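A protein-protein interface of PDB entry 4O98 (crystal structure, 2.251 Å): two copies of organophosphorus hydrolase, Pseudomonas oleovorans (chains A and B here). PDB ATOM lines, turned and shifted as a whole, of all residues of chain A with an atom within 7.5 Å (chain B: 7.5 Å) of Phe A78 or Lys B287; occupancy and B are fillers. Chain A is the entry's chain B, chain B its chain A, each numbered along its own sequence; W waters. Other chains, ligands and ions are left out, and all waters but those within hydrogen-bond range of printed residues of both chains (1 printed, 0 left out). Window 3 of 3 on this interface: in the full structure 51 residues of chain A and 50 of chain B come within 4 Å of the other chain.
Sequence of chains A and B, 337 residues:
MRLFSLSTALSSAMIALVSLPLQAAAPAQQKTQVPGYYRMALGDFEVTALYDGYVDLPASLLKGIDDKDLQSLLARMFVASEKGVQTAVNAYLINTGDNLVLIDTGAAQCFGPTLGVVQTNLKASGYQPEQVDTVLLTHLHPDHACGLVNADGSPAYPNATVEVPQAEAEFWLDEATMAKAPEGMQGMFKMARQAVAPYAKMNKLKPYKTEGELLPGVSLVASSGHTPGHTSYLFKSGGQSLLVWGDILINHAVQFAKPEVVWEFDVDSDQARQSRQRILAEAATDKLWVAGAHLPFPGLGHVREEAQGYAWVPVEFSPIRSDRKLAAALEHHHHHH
OE2 of Glu B316 is in hydrogen-bond range of NE2 of His A252 (2.6 Å). NH1 of Arg B304 sits at hydrogen-bond distance from O of Arg A76, 2.8 Å away. The guanidinium group of Arg B304 sits at hydrogen-bond distance from the side-chain sulfur of Met A77.
The backbone NH (N) of Ala B311 sits at hydrogen-bond distance from the backbone carbonyl oxygen (O) of Arg B304, at 2.9 Å. The backbone carbonyl oxygen (O) of Leu A74 is in hydrogen-bond range of the backbone NH (N) of Val A79 (2.9 Å). The backbone carbonyl oxygen of Val B313 is in hydrogen-bond range of the backbone NH of His B302, at 2.9 Å.
Among the printed residues, pairs that only touch across the chains: Val A79 with Glu B316, Phe A78 with His B302, Met A77 with Val B313, Phe A78 with Lys B287 and Phe A78 with Val B303.
Printed residues of chain B within 4 Å of Phe A78: Lys B287, His B302 and Val B303. Of chain A, only Phe A78 comes within 4 Å of Lys B287. Printed residues of chain A within 4 Å of Val B313: Met A77. Printed residues of chain B within 4 Å of Met A77: Arg B304 (3.5 Å) and Val B313 (3.7 Å). Ser A72 touches none of the printed residues of chain B.
Of the 12 printed residues of chain A, 5 touch a printed residue of chain B. Printed residues of chain A that touch a printed residue of chain B: Arg A76, Met A77, Phe A78, Val A79 and His A252. Hydrophobic or aromatic side chains of chain A that line the printed part of chain B: Met A77, Phe A78, Val A79 and His A252. Of the 21 printed residues of chain B, 6 touch a printed residue of chain A. Hydrophobic or aromatic side chains of chain B that line the printed part of chain A: His B302 and Val B313. Among the printed residues, 8 pairs touch across the chains. Among the printed residues, no Asp or Glu carboxylate lies within 4 Å of a Lys or Arg side-chain nitrogen of the other chain.
No position is printed for both chains. Of the 8 pairs that touch across the chains among the printed residues, none has its exchanged pair printed and touching as well.
Water W1 lies within hydrogen-bond range of the side-chain carboxylate of Glu B316 (2.5 Å) and the backbone carbonyl oxygen of Met A77 (2.7 Å).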
ATOM      1  N   SER A  72     -28.813   3.084 -21.641  1.00  0.00           N
ATOM      2  CA  SER A  72     -28.772   3.601 -23.004  1.00  0.00           C
ATOM      3  C   SER A  72     -28.001   4.924 -23.061  1.00  0.00           C
ATOM      4  O   SER A  72     -27.222   5.168 -23.987  1.00  0.00           O
ATOM      5  CB  SER A  72     -30.185   3.781 -23.541  1.00  0.00           C
ATOM      6  OG  SER A  72     -30.131   4.398 -24.806  1.00  0.00           O
ATOM      7  N   LEU A  73     -28.216   5.770 -22.058  1.00  0.00           N
ATOM      8  CA  LEU A  73     -27.518   7.055 -21.966  1.00  0.00           C
ATOM      9  C   LEU A  73     -26.034   6.852 -21.688  1.00  0.00           C
ATOM     10  O   LEU A  73     -25.190   7.553 -22.252  1.00  0.00           O
ATOM     11  CB  LEU A  73     -28.142   7.923 -20.871  1.00  0.00           C
ATOM     12  CG  LEU A  73     -29.425   8.645 -21.274  1.00  0.00           C
ATOM     13  CD1 LEU A  73     -30.123   9.273 -20.061  1.00  0.00           C
ATOM     14  CD2 LEU A  73     -29.102   9.709 -22.333  1.00  0.00           C
ATOM     15  N   LEU A  74     -25.720   5.897 -20.814  1.00  0.00           N
ATOM     16  CA  LEU A  74     -24.327   5.558 -20.527  1.00  0.00           C
ATOM     17  C   LEU A  74     -23.638   4.941 -21.748  1.00  0.00           C
ATOM     18  O   LEU A  74     -22.481   5.262 -22.048  1.00  0.00           O
ATOM     19  CB  LEU A  74     -24.229   4.601 -19.338  1.00  0.00           C
ATOM     20  CG  LEU A  74     -24.756   5.098 -17.996  1.00  0.00           C
ATOM     21  CD1 LEU A  74     -24.773   3.950 -16.995  1.00  0.00           C
ATOM     22  CD2 LEU A  74     -23.896   6.234 -17.481  1.00  0.00           C
ATOM     23  N   ALA A  75     -24.344   4.054 -22.444  1.00  0.00           N
ATOM     24  CA  ALA A  75     -23.766   3.395 -23.605  1.00  0.00           C
ATOM     25  C   ALA A  75     -23.513   4.355 -24.756  1.00  0.00           C
ATOM     26  O   ALA A  75     -22.542   4.181 -25.479  1.00  0.00           O
ATOM     27  CB  ALA A  75     -24.617   2.220 -24.068  1.00  0.00           C
ATOM     28  N   ARG A  76     -24.358   5.367 -24.938  1.00  0.00           N
ATOM     29  CA  ARG A  76     -24.124   6.260 -26.076  1.00  0.00           C
ATOM     30  C   ARG A  76     -22.900   7.152 -25.834  1.00  0.00           C
ATOM     31  O   ARG A  76     -22.362   7.734 -26.767  1.00  0.00           O
ATOM     32  CB  ARG A  76     -25.370   7.073 -26.454  1.00  0.00           C
ATOM     33  CG  ARG A  76     -25.578   8.332 -25.646  1.00  0.00           C
ATOM     34  CD  ARG A  76     -26.915   9.031 -25.971  1.00  0.00           C
ATOM     35  NE  ARG A  76     -26.771  10.164 -26.890  1.00  0.00           N
ATOM     36  CZ  ARG A  76     -26.278  11.352 -26.542  1.00  0.00           C
ATOM     37  NH1 ARG A  76     -26.195  12.331 -27.441  1.00  0.00           N
ATOM     38  NH2 ARG A  76     -25.862  11.566 -25.291  1.00  0.00           N
ATOM     39  N   MET A  77     -22.451   7.247 -24.584  1.00  0.00           N
ATOM     40  CA  MET A  77     -21.202   7.964 -24.285  1.00  0.00           C
ATOM     41  C   MET A  77     -20.074   6.984 -23.984  1.00  0.00           C
ATOM     42  O   MET A  77     -19.030   7.367 -23.452  1.00  0.00           O
ATOM     43  CB  MET A  77     -21.378   8.914 -23.107  1.00  0.00           C
ATOM     44  CG  MET A  77     -22.308  10.092 -23.397  1.00  0.00           C
ATOM     45  SD  MET A  77     -21.784  11.186 -24.733  1.00  0.00           S
ATOM     46  CE  MET A  77     -20.252  11.844 -24.071  1.00  0.00           C
ATOM     47  N   PHE A  78     -20.298   5.719 -24.325  1.00  0.00           N
ATOM     48  CA  PHE A  78     -19.295   4.667 -24.160  1.00  0.00           C
ATOM     49  C   PHE A  78     -18.772   4.574 -22.730  1.00  0.00           C
ATOM     50  O   PHE A  78     -17.601   4.291 -22.496  1.00  0.00           O
ATOM     51  CB  PHE A  78     -18.176   4.831 -25.201  1.00  0.00           C
ATOM     52  CG  PHE A  78     -18.674   4.667 -26.618  1.00  0.00           C
ATOM     53  CD1 PHE A  78     -19.218   5.744 -27.306  1.00  0.00           C
ATOM     54  CD2 PHE A  78     -18.642   3.426 -27.245  1.00  0.00           C
ATOM     55  CE1 PHE A  78     -19.711   5.594 -28.602  1.00  0.00           C
ATOM     56  CE2 PHE A  78     -19.131   3.266 -28.543  1.00  0.00           C
ATOM     57  CZ  PHE A  78     -19.670   4.349 -29.224  1.00  0.00           C
ATOM     58  N   VAL A  79     -19.670   4.818 -21.782  1.00  0.00           N
ATOM     59  CA  VAL A  79     -19.366   4.707 -20.364  1.00  0.00           C
ATOM     60  C   VAL A  79     -19.774   3.333 -19.865  1.00  0.00           C
ATOM     61  O   VAL A  79     -20.945   2.969 -19.959  1.00  0.00           O
ATOM     62  CB  VAL A  79     -20.149   5.744 -19.557  1.00  0.00           C
ATOM     63  CG1 VAL A  79     -19.911   5.537 -18.053  1.00  0.00           C
ATOM     64  CG2 VAL A  79     -19.771   7.158 -20.009  1.00  0.00           C
ATOM     65  N   ALA A  80     -18.818   2.567 -19.339  1.00  0.00           N
ATOM     66  CA  ALA A  80     -19.132   1.257 -18.767  1.00  0.00           C
ATOM     67  C   ALA A  80     -19.687   1.435 -17.355  1.00  0.00           C
ATOM     68  O   ALA A  80     -19.115   2.154 -16.532  1.00  0.00           O
ATOM     69  CB  ALA A  80     -17.902   0.350 -18.764  1.00  0.00           C
ATOM     70  N   SER A  81     -20.842   0.835 -17.107  1.00  0.00           N
ATOM     71  CA  SER A  81     -21.386   0.700 -15.761  1.00  0.00           C
ATOM     72  C   SER A  81     -21.120  -0.767 -15.567  1.00  0.00           C
ATOM     73  O   SER A  81     -20.446  -1.344 -16.421  1.00  0.00           O
ATOM     74  CB  SER A  81     -22.876   1.016 -15.746  1.00  0.00           C
ATOM     75  OG  SER A  81     -23.554   0.303 -16.766  1.00  0.00           O
ATOM     76  N   HIS A 252     -21.845  13.080 -16.332  1.00  0.00           N
ATOM     77  CA  HIS A 252     -21.978  13.897 -17.541  1.00  0.00           C
ATOM     78  C   HIS A 252     -22.870  13.234 -18.591  1.00  0.00           C
ATOM     79  O   HIS A 252     -23.574  13.911 -19.330  1.00  0.00           O
ATOM     80  CB  HIS A 252     -20.597  14.189 -18.149  1.00  0.00           C
ATOM     81  CG  HIS A 252     -19.930  12.975 -18.723  1.00  0.00           C
ATOM     82  ND1 HIS A 252     -19.887  12.724 -20.081  1.00  0.00           N
ATOM     83  CD2 HIS A 252     -19.323  11.922 -18.122  1.00  0.00           C
ATOM     84  CE1 HIS A 252     -19.262  11.578 -20.293  1.00  0.00           C
ATOM     85  NE2 HIS A 252     -18.909  11.069 -19.123  1.00  0.00           N
ATOM     86  N   ALA A 253     -22.844  11.909 -18.644  1.00  0.00           N
ATOM     87  CA  ALA A 253     -23.545  11.173 -19.693  1.00  0.00           C
ATOM     88  C   ALA A 253     -25.066  11.160 -19.530  1.00  0.00           C
ATOM     89  O   ALA A 253     -25.792  10.950 -20.504  1.00  0.00           O
ATOM     90  CB  ALA A 253     -23.017   9.757 -19.786  1.00  0.00           C
ATOM     91  N   SER B 241     -10.194  -3.435 -30.384  1.00  0.00           N
ATOM     92  CA  SER B 241      -9.705  -2.951 -31.668  1.00  0.00           C
ATOM     93  C   SER B 241      -9.446  -1.441 -31.641  1.00  0.00           C
ATOM     94  O   SER B 241     -10.244  -0.675 -31.074  1.00  0.00           O
ATOM     95  CB  SER B 241     -10.727  -3.282 -32.749  1.00  0.00           C
ATOM     96  OG  SER B 241     -11.012  -4.670 -32.769  1.00  0.00           O
ATOM     97  N   ALA B 281     -19.041   4.709 -40.908  1.00  0.00           N
ATOM     98  CA  ALA B 281     -20.142   3.774 -40.698  1.00  0.00           C
ATOM     99  C   ALA B 281     -19.670   2.499 -39.995  1.00  0.00           C
ATOM    100  O   ALA B 281     -20.341   1.998 -39.100  1.00  0.00           O
ATOM    101  CB  ALA B 281     -20.838   3.452 -42.034  1.00  0.00           C
ATOM    102  N   GLU B 282     -18.512   1.984 -40.397  1.00  0.00           N
ATOM    103  CA  GLU B 282     -17.977   0.757 -39.815  1.00  0.00           C
ATOM    104  C   GLU B 282     -17.526   0.973 -38.379  1.00  0.00           C
ATOM    105  O   GLU B 282     -17.773   0.128 -37.507  1.00  0.00           O
ATOM    106  CB  GLU B 282     -16.807   0.220 -40.641  1.00  0.00           C
ATOM    107  CG  GLU B 282     -17.167  -0.166 -42.076  1.00  0.00           C
ATOM    108  CD  GLU B 282     -18.264  -1.223 -42.163  1.00  0.00           C
ATOM    109  OE1 GLU B 282     -17.930  -2.424 -42.144  1.00  0.00           O
ATOM    110  OE2 GLU B 282     -19.457  -0.855 -42.266  1.00  0.00           O
ATOM    111  N   ALA B 283     -16.856   2.098 -38.139  1.00  0.00           N
ATOM    112  CA  ALA B 283     -16.398   2.424 -36.793  1.00  0.00           C
ATOM    113  C   ALA B 283     -17.587   2.586 -35.857  1.00  0.00           C
ATOM    114  O   ALA B 283     -17.556   2.126 -34.717  1.00  0.00           O
ATOM    115  CB  ALA B 283     -15.564   3.684 -36.806  1.00  0.00           C
ATOM    116  N   ALA B 284     -18.631   3.253 -36.342  1.00  0.00           N
ATOM    117  CA  ALA B 284     -19.826   3.453 -35.532  1.00  0.00           C
ATOM    118  C   ALA B 284     -20.506   2.123 -35.185  1.00  0.00           C
ATOM    119  O   ALA B 284     -20.883   1.905 -34.033  1.00  0.00           O
ATOM    120  CB  ALA B 284     -20.797   4.390 -36.222  1.00  0.00           C
ATOM    121  N   THR B 285     -20.654   1.239 -36.173  1.00  0.00           N
ATOM    122  CA  THR B 285     -21.351  -0.030 -35.942  1.00  0.00           C
ATOM    123  C   THR B 285     -20.504  -1.117 -35.258  1.00  0.00           C
ATOM    124  O   THR B 285     -21.058  -1.944 -34.541  1.00  0.00           O
ATOM    125  CB  THR B 285     -22.042  -0.588 -37.217  1.00  0.00           C
ATOM    126  OG1 THR B 285     -21.061  -0.989 -38.184  1.00  0.00           O
ATOM    127  CG2 THR B 285     -22.970   0.454 -37.824  1.00  0.00           C
ATOM    128  N   ASP B 286     -19.183  -1.115 -35.450  1.00  0.00           N
ATOM    129  CA  ASP B 286     -18.319  -2.044 -34.702  1.00  0.00           C
ATOM    130  C   ASP B 286     -17.982  -1.528 -33.303  1.00  0.00           C
ATOM    131  O   ASP B 286     -17.526  -2.291 -32.449  1.00  0.00           O
ATOM    132  CB  ASP B 286     -17.002  -2.318 -35.435  1.00  0.00           C
ATOM    133  CG  ASP B 286     -17.201  -2.908 -36.821  1.00  0.00           C
ATOM    134  OD1 ASP B 286     -18.334  -3.347 -37.134  1.00  0.00           O
ATOM    135  OD2 ASP B 286     -16.209  -2.931 -37.588  1.00  0.00           O
ATOM    136  N   LYS B 287     -18.183  -0.232 -33.080  1.00  0.00           N
ATOM    137  CA  LYS B 287     -17.794   0.415 -31.820  1.00  0.00           C
ATOM    138  C   LYS B 287     -16.308   0.250 -31.463  1.00  0.00           C
ATOM    139  O   LYS B 287     -15.964   0.120 -30.283  1.00  0.00           O
ATOM    140  CB  LYS B 287     -18.646  -0.090 -30.649  1.00  0.00           C
ATOM    141  CG  LYS B 287     -20.109   0.348 -30.654  1.00  0.00           C
ATOM    142  CD  LYS B 287     -20.751  -0.081 -29.325  1.00  0.00           C
ATOM    143  CE  LYS B 287     -22.250   0.199 -29.271  1.00  0.00           C
ATOM    144  NZ  LYS B 287     -22.862  -0.599 -28.160  1.00  0.00           N
ATOM    145  N   LEU B 288     -15.426   0.251 -32.460  1.00  0.00           N
ATOM    146  CA  LEU B 288     -13.993   0.182 -32.167  1.00  0.00           C
ATOM    147  C   LEU B 288     -13.400   1.523 -31.721  1.00  0.00           C
ATOM    148  O   LEU B 288     -13.993   2.585 -31.944  1.00  0.00           O
ATOM    149  CB  LEU B 288     -13.204  -0.404 -33.344  1.00  0.00           C
ATOM    150  CG  LEU B 288     -13.367   0.037 -34.801  1.00  0.00           C
ATOM    151  CD1 LEU B 288     -13.292   1.530 -34.970  1.00  0.00           C
ATOM    152  CD2 LEU B 288     -12.254  -0.594 -35.605  1.00  0.00           C
ATOM    153  N   TRP B 289     -12.231   1.471 -31.089  1.00  0.00           N
ATOM    154  CA  TRP B 289     -11.502   2.690 -30.747  1.00  0.00           C
ATOM    155  C   TRP B 289     -10.922   3.331 -32.015  1.00  0.00           C
ATOM    156  O   TRP B 289     -10.533   2.626 -32.949  1.00  0.00           O
ATOM    157  CB  TRP B 289     -10.355   2.372 -29.788  1.00  0.00           C
ATOM    158  CG  TRP B 289     -10.802   1.995 -28.422  1.00  0.00           C
ATOM    159  CD1 TRP B 289     -10.981   0.727 -27.928  1.00  0.00           C
ATOM    160  CD2 TRP B 289     -11.112   2.892 -27.353  1.00  0.00           C
ATOM    161  NE1 TRP B 289     -11.392   0.790 -26.621  1.00  0.00           N
ATOM    162  CE2 TRP B 289     -11.482   2.105 -26.243  1.00  0.00           C
ATOM    163  CE3 TRP B 289     -11.115   4.282 -27.229  1.00  0.00           C
ATOM    164  CZ2 TRP B 289     -11.858   2.669 -25.025  1.00  0.00           C
ATOM    165  CZ3 TRP B 289     -11.492   4.840 -26.025  1.00  0.00           C
ATOM    166  CH2 TRP B 289     -11.846   4.039 -24.932  1.00  0.00           C
ATOM    167  N   VAL B 290     -10.874   4.663 -32.043  1.00  0.00           N
ATOM    168  CA  VAL B 290     -10.255   5.405 -33.148  1.00  0.00           C
ATOM    169  C   VAL B 290      -9.140   6.275 -32.575  1.00  0.00           C
ATOM    170  O   VAL B 290      -9.260   6.825 -31.473  1.00  0.00           O
ATOM    171  CB  VAL B 290     -11.281   6.296 -33.921  1.00  0.00           C
ATOM    172  CG1 VAL B 290     -10.575   7.208 -34.943  1.00  0.00           C
ATOM    173  CG2 VAL B 290     -12.350   5.444 -34.621  1.00  0.00           C
ATOM    174  N   GLY B 301     -10.905   7.823 -29.061  1.00  0.00           N
ATOM    175  CA  GLY B 301     -12.311   7.744 -28.698  1.00  0.00           C
ATOM    176  C   GLY B 301     -13.134   6.877 -29.631  1.00  0.00           C
ATOM    177  O   GLY B 301     -12.598   6.002 -30.321  1.00  0.00           O
ATOM    178  N   HIS B 302     -14.441   7.116 -29.660  1.00  0.00           N
ATOM    179  CA  HIS B 302     -15.327   6.307 -30.490  1.00  0.00           C
ATOM    180  C   HIS B 302     -16.178   7.172 -31.422  1.00  0.00           C
ATOM    181  O   HIS B 302     -16.399   8.352 -31.159  1.00  0.00           O
ATOM    182  CB  HIS B 302     -16.265   5.474 -29.604  1.00  0.00           C
ATOM    183  CG  HIS B 302     -15.572   4.440 -28.778  1.00  0.00           C
ATOM    184  ND1 HIS B 302     -15.045   4.710 -27.527  1.00  0.00           N
ATOM    185  CD2 HIS B 302     -15.348   3.122 -29.006  1.00  0.00           C
ATOM    186  CE1 HIS B 302     -14.523   3.602 -27.029  1.00  0.00           C
ATOM    187  NE2 HIS B 302     -14.693   2.627 -27.904  1.00  0.00           N
ATOM    188  N   VAL B 303     -16.679   6.566 -32.493  1.00  0.00           N
ATOM    189  CA  VAL B 303     -17.646   7.221 -33.368  1.00  0.00           C
ATOM    190  C   VAL B 303     -19.051   6.691 -33.048  1.00  0.00           C
ATOM    191  O   VAL B 303     -19.268   5.479 -32.955  1.00  0.00           O
ATOM    192  CB  VAL B 303     -17.345   6.960 -34.868  1.00  0.00           C
ATOM    193  CG1 VAL B 303     -18.334   7.711 -35.754  1.00  0.00           C
ATOM    194  CG2 VAL B 303     -15.881   7.334 -35.231  1.00  0.00           C
ATOM    195  N   ARG B 304     -20.005   7.603 -32.888  1.00  0.00           N
ATOM    196  CA  ARG B 304     -21.396   7.222 -32.653  1.00  0.00           C
ATOM    197  C   ARG B 304     -22.262   7.698 -33.813  1.00  0.00           C
ATOM    198  O   ARG B 304     -22.143   8.848 -34.238  1.00  0.00           O
ATOM    199  CB  ARG B 304     -21.897   7.883 -31.369  1.00  0.00           C
ATOM    200  CG  ARG B 304     -23.302   7.507 -30.983  1.00  0.00           C
ATOM    201  CD  ARG B 304     -23.705   8.225 -29.700  1.00  0.00           C
ATOM    202  NE  ARG B 304     -23.922   9.655 -29.901  1.00  0.00           N
ATOM    203  CZ  ARG B 304     -23.461  10.594 -29.078  1.00  0.00           C
ATOM    204  NH1 ARG B 304     -22.752  10.247 -28.009  1.00  0.00           N
ATOM    205  NH2 ARG B 304     -23.704  11.874 -29.322  1.00  0.00           N
ATOM    206  N   GLU B 305     -23.145   6.837 -34.316  1.00  0.00           N
ATOM    207  CA  GLU B 305     -24.090   7.269 -35.343  1.00  0.00           C
ATOM    208  C   GLU B 305     -25.160   8.160 -34.737  1.00  0.00           C
ATOM    209  O   GLU B 305     -25.720   7.826 -33.696  1.00  0.00           O
ATOM    210  CB  GLU B 305     -24.752   6.079 -36.041  1.00  0.00           C
ATOM    211  CG  GLU B 305     -25.731   6.519 -37.133  1.00  0.00           C
ATOM    212  CD  GLU B 305     -26.377   5.365 -37.891  1.00  0.00           C
ATOM    213  OE1 GLU B 305     -25.761   4.283 -38.000  1.00  0.00           O
ATOM    214  OE2 GLU B 305     -27.506   5.561 -38.391  1.00  0.00           O
ATOM    215  N   ALA B 311     -21.113  11.502 -34.502  1.00  0.00           N
ATOM    216  CA  ALA B 311     -20.551  12.337 -33.444  1.00  0.00           C
ATOM    217  C   ALA B 311     -19.311  11.669 -32.885  1.00  0.00           C
ATOM    218  O   ALA B 311     -19.192  10.438 -32.906  1.00  0.00           O
ATOM    219  CB  ALA B 311     -21.572  12.586 -32.337  1.00  0.00           C
ATOM    220  N   TRP B 312     -18.390  12.486 -32.386  1.00  0.00           N
ATOM    221  CA  TRP B 312     -17.149  11.990 -31.818  1.00  0.00           C
ATOM    222  C   TRP B 312     -17.257  11.956 -30.298  1.00  0.00           C
ATOM    223  O   TRP B 312     -17.677  12.928 -29.686  1.00  0.00           O
ATOM    224  CB  TRP B 312     -15.992  12.894 -32.259  1.00  0.00           C
ATOM    225  CG  TRP B 312     -14.658  12.598 -31.599  1.00  0.00           C
ATOM    226  CD1 TRP B 312     -13.966  13.410 -30.732  1.00  0.00           C
ATOM    227  CD2 TRP B 312     -13.853  11.421 -31.772  1.00  0.00           C
ATOM    228  NE1 TRP B 312     -12.786  12.802 -30.354  1.00  0.00           N
ATOM    229  CE2 TRP B 312     -12.693  11.583 -30.976  1.00  0.00           C
ATOM    230  CE3 TRP B 312     -14.003  10.249 -32.511  1.00  0.00           C
ATOM    231  CZ2 TRP B 312     -11.687  10.605 -30.908  1.00  0.00           C
ATOM    232  CZ3 TRP B 312     -13.007   9.281 -32.440  1.00  0.00           C
ATOM    233  CH2 TRP B 312     -11.860   9.470 -31.650  1.00  0.00           C
ATOM    234  N   VAL B 313     -16.886  10.829 -29.700  1.00  0.00           N
ATOM    235  CA  VAL B 313     -16.898  10.673 -28.244  1.00  0.00           C
ATOM    236  C   VAL B 313     -15.479  10.390 -27.744  1.00  0.00           C
ATOM    237  O   VAL B 313     -14.984   9.272 -27.859  1.00  0.00           O
ATOM    238  CB  VAL B 313     -17.813   9.500 -27.812  1.00  0.00           C
ATOM    239  CG1 VAL B 313     -17.829   9.373 -26.294  1.00  0.00           C
ATOM    240  CG2 VAL B 313     -19.237   9.692 -28.343  1.00  0.00           C
ATOM    241  N   PRO B 314     -14.815  11.406 -27.180  1.00  0.00           N
ATOM    242  CA  PRO B 314     -13.411  11.240 -26.769  1.00  0.00           C
ATOM    243  C   PRO B 314     -13.249  10.404 -25.504  1.00  0.00           C
ATOM    244  O   PRO B 314     -14.172  10.437 -24.666  1.00  0.00           O
ATOM    245  CB  PRO B 314     -12.953  12.684 -26.503  1.00  0.00           C
ATOM    246  CG  PRO B 314     -14.226  13.436 -26.165  1.00  0.00           C
ATOM    247  CD  PRO B 314     -15.307  12.789 -27.000  1.00  0.00           C
ATOM    248  N   GLU B 316     -12.383   9.306 -21.799  1.00  0.00           N
ATOM    249  CA  GLU B 316     -12.329  10.017 -20.546  1.00  0.00           C
ATOM    250  C   GLU B 316     -10.970   9.745 -19.906  1.00  0.00           C
ATOM    251  O   GLU B 316     -10.527   8.594 -19.836  1.00  0.00           O
ATOM    252  CB  GLU B 316     -13.463   9.541 -19.651  1.00  0.00           C
ATOM    253  CG  GLU B 316     -14.832   9.785 -20.281  1.00  0.00           C
ATOM    254  CD  GLU B 316     -15.946   9.486 -19.317  1.00  0.00           C
ATOM    255  OE1 GLU B 316     -15.638   9.388 -18.110  1.00  0.00           O
ATOM    256  OE2 GLU B 316     -17.113   9.345 -19.754  1.00  0.00           O
HETATM  257  O   HOH W   1     -17.685   9.371 -22.220  1.00  0.00           O
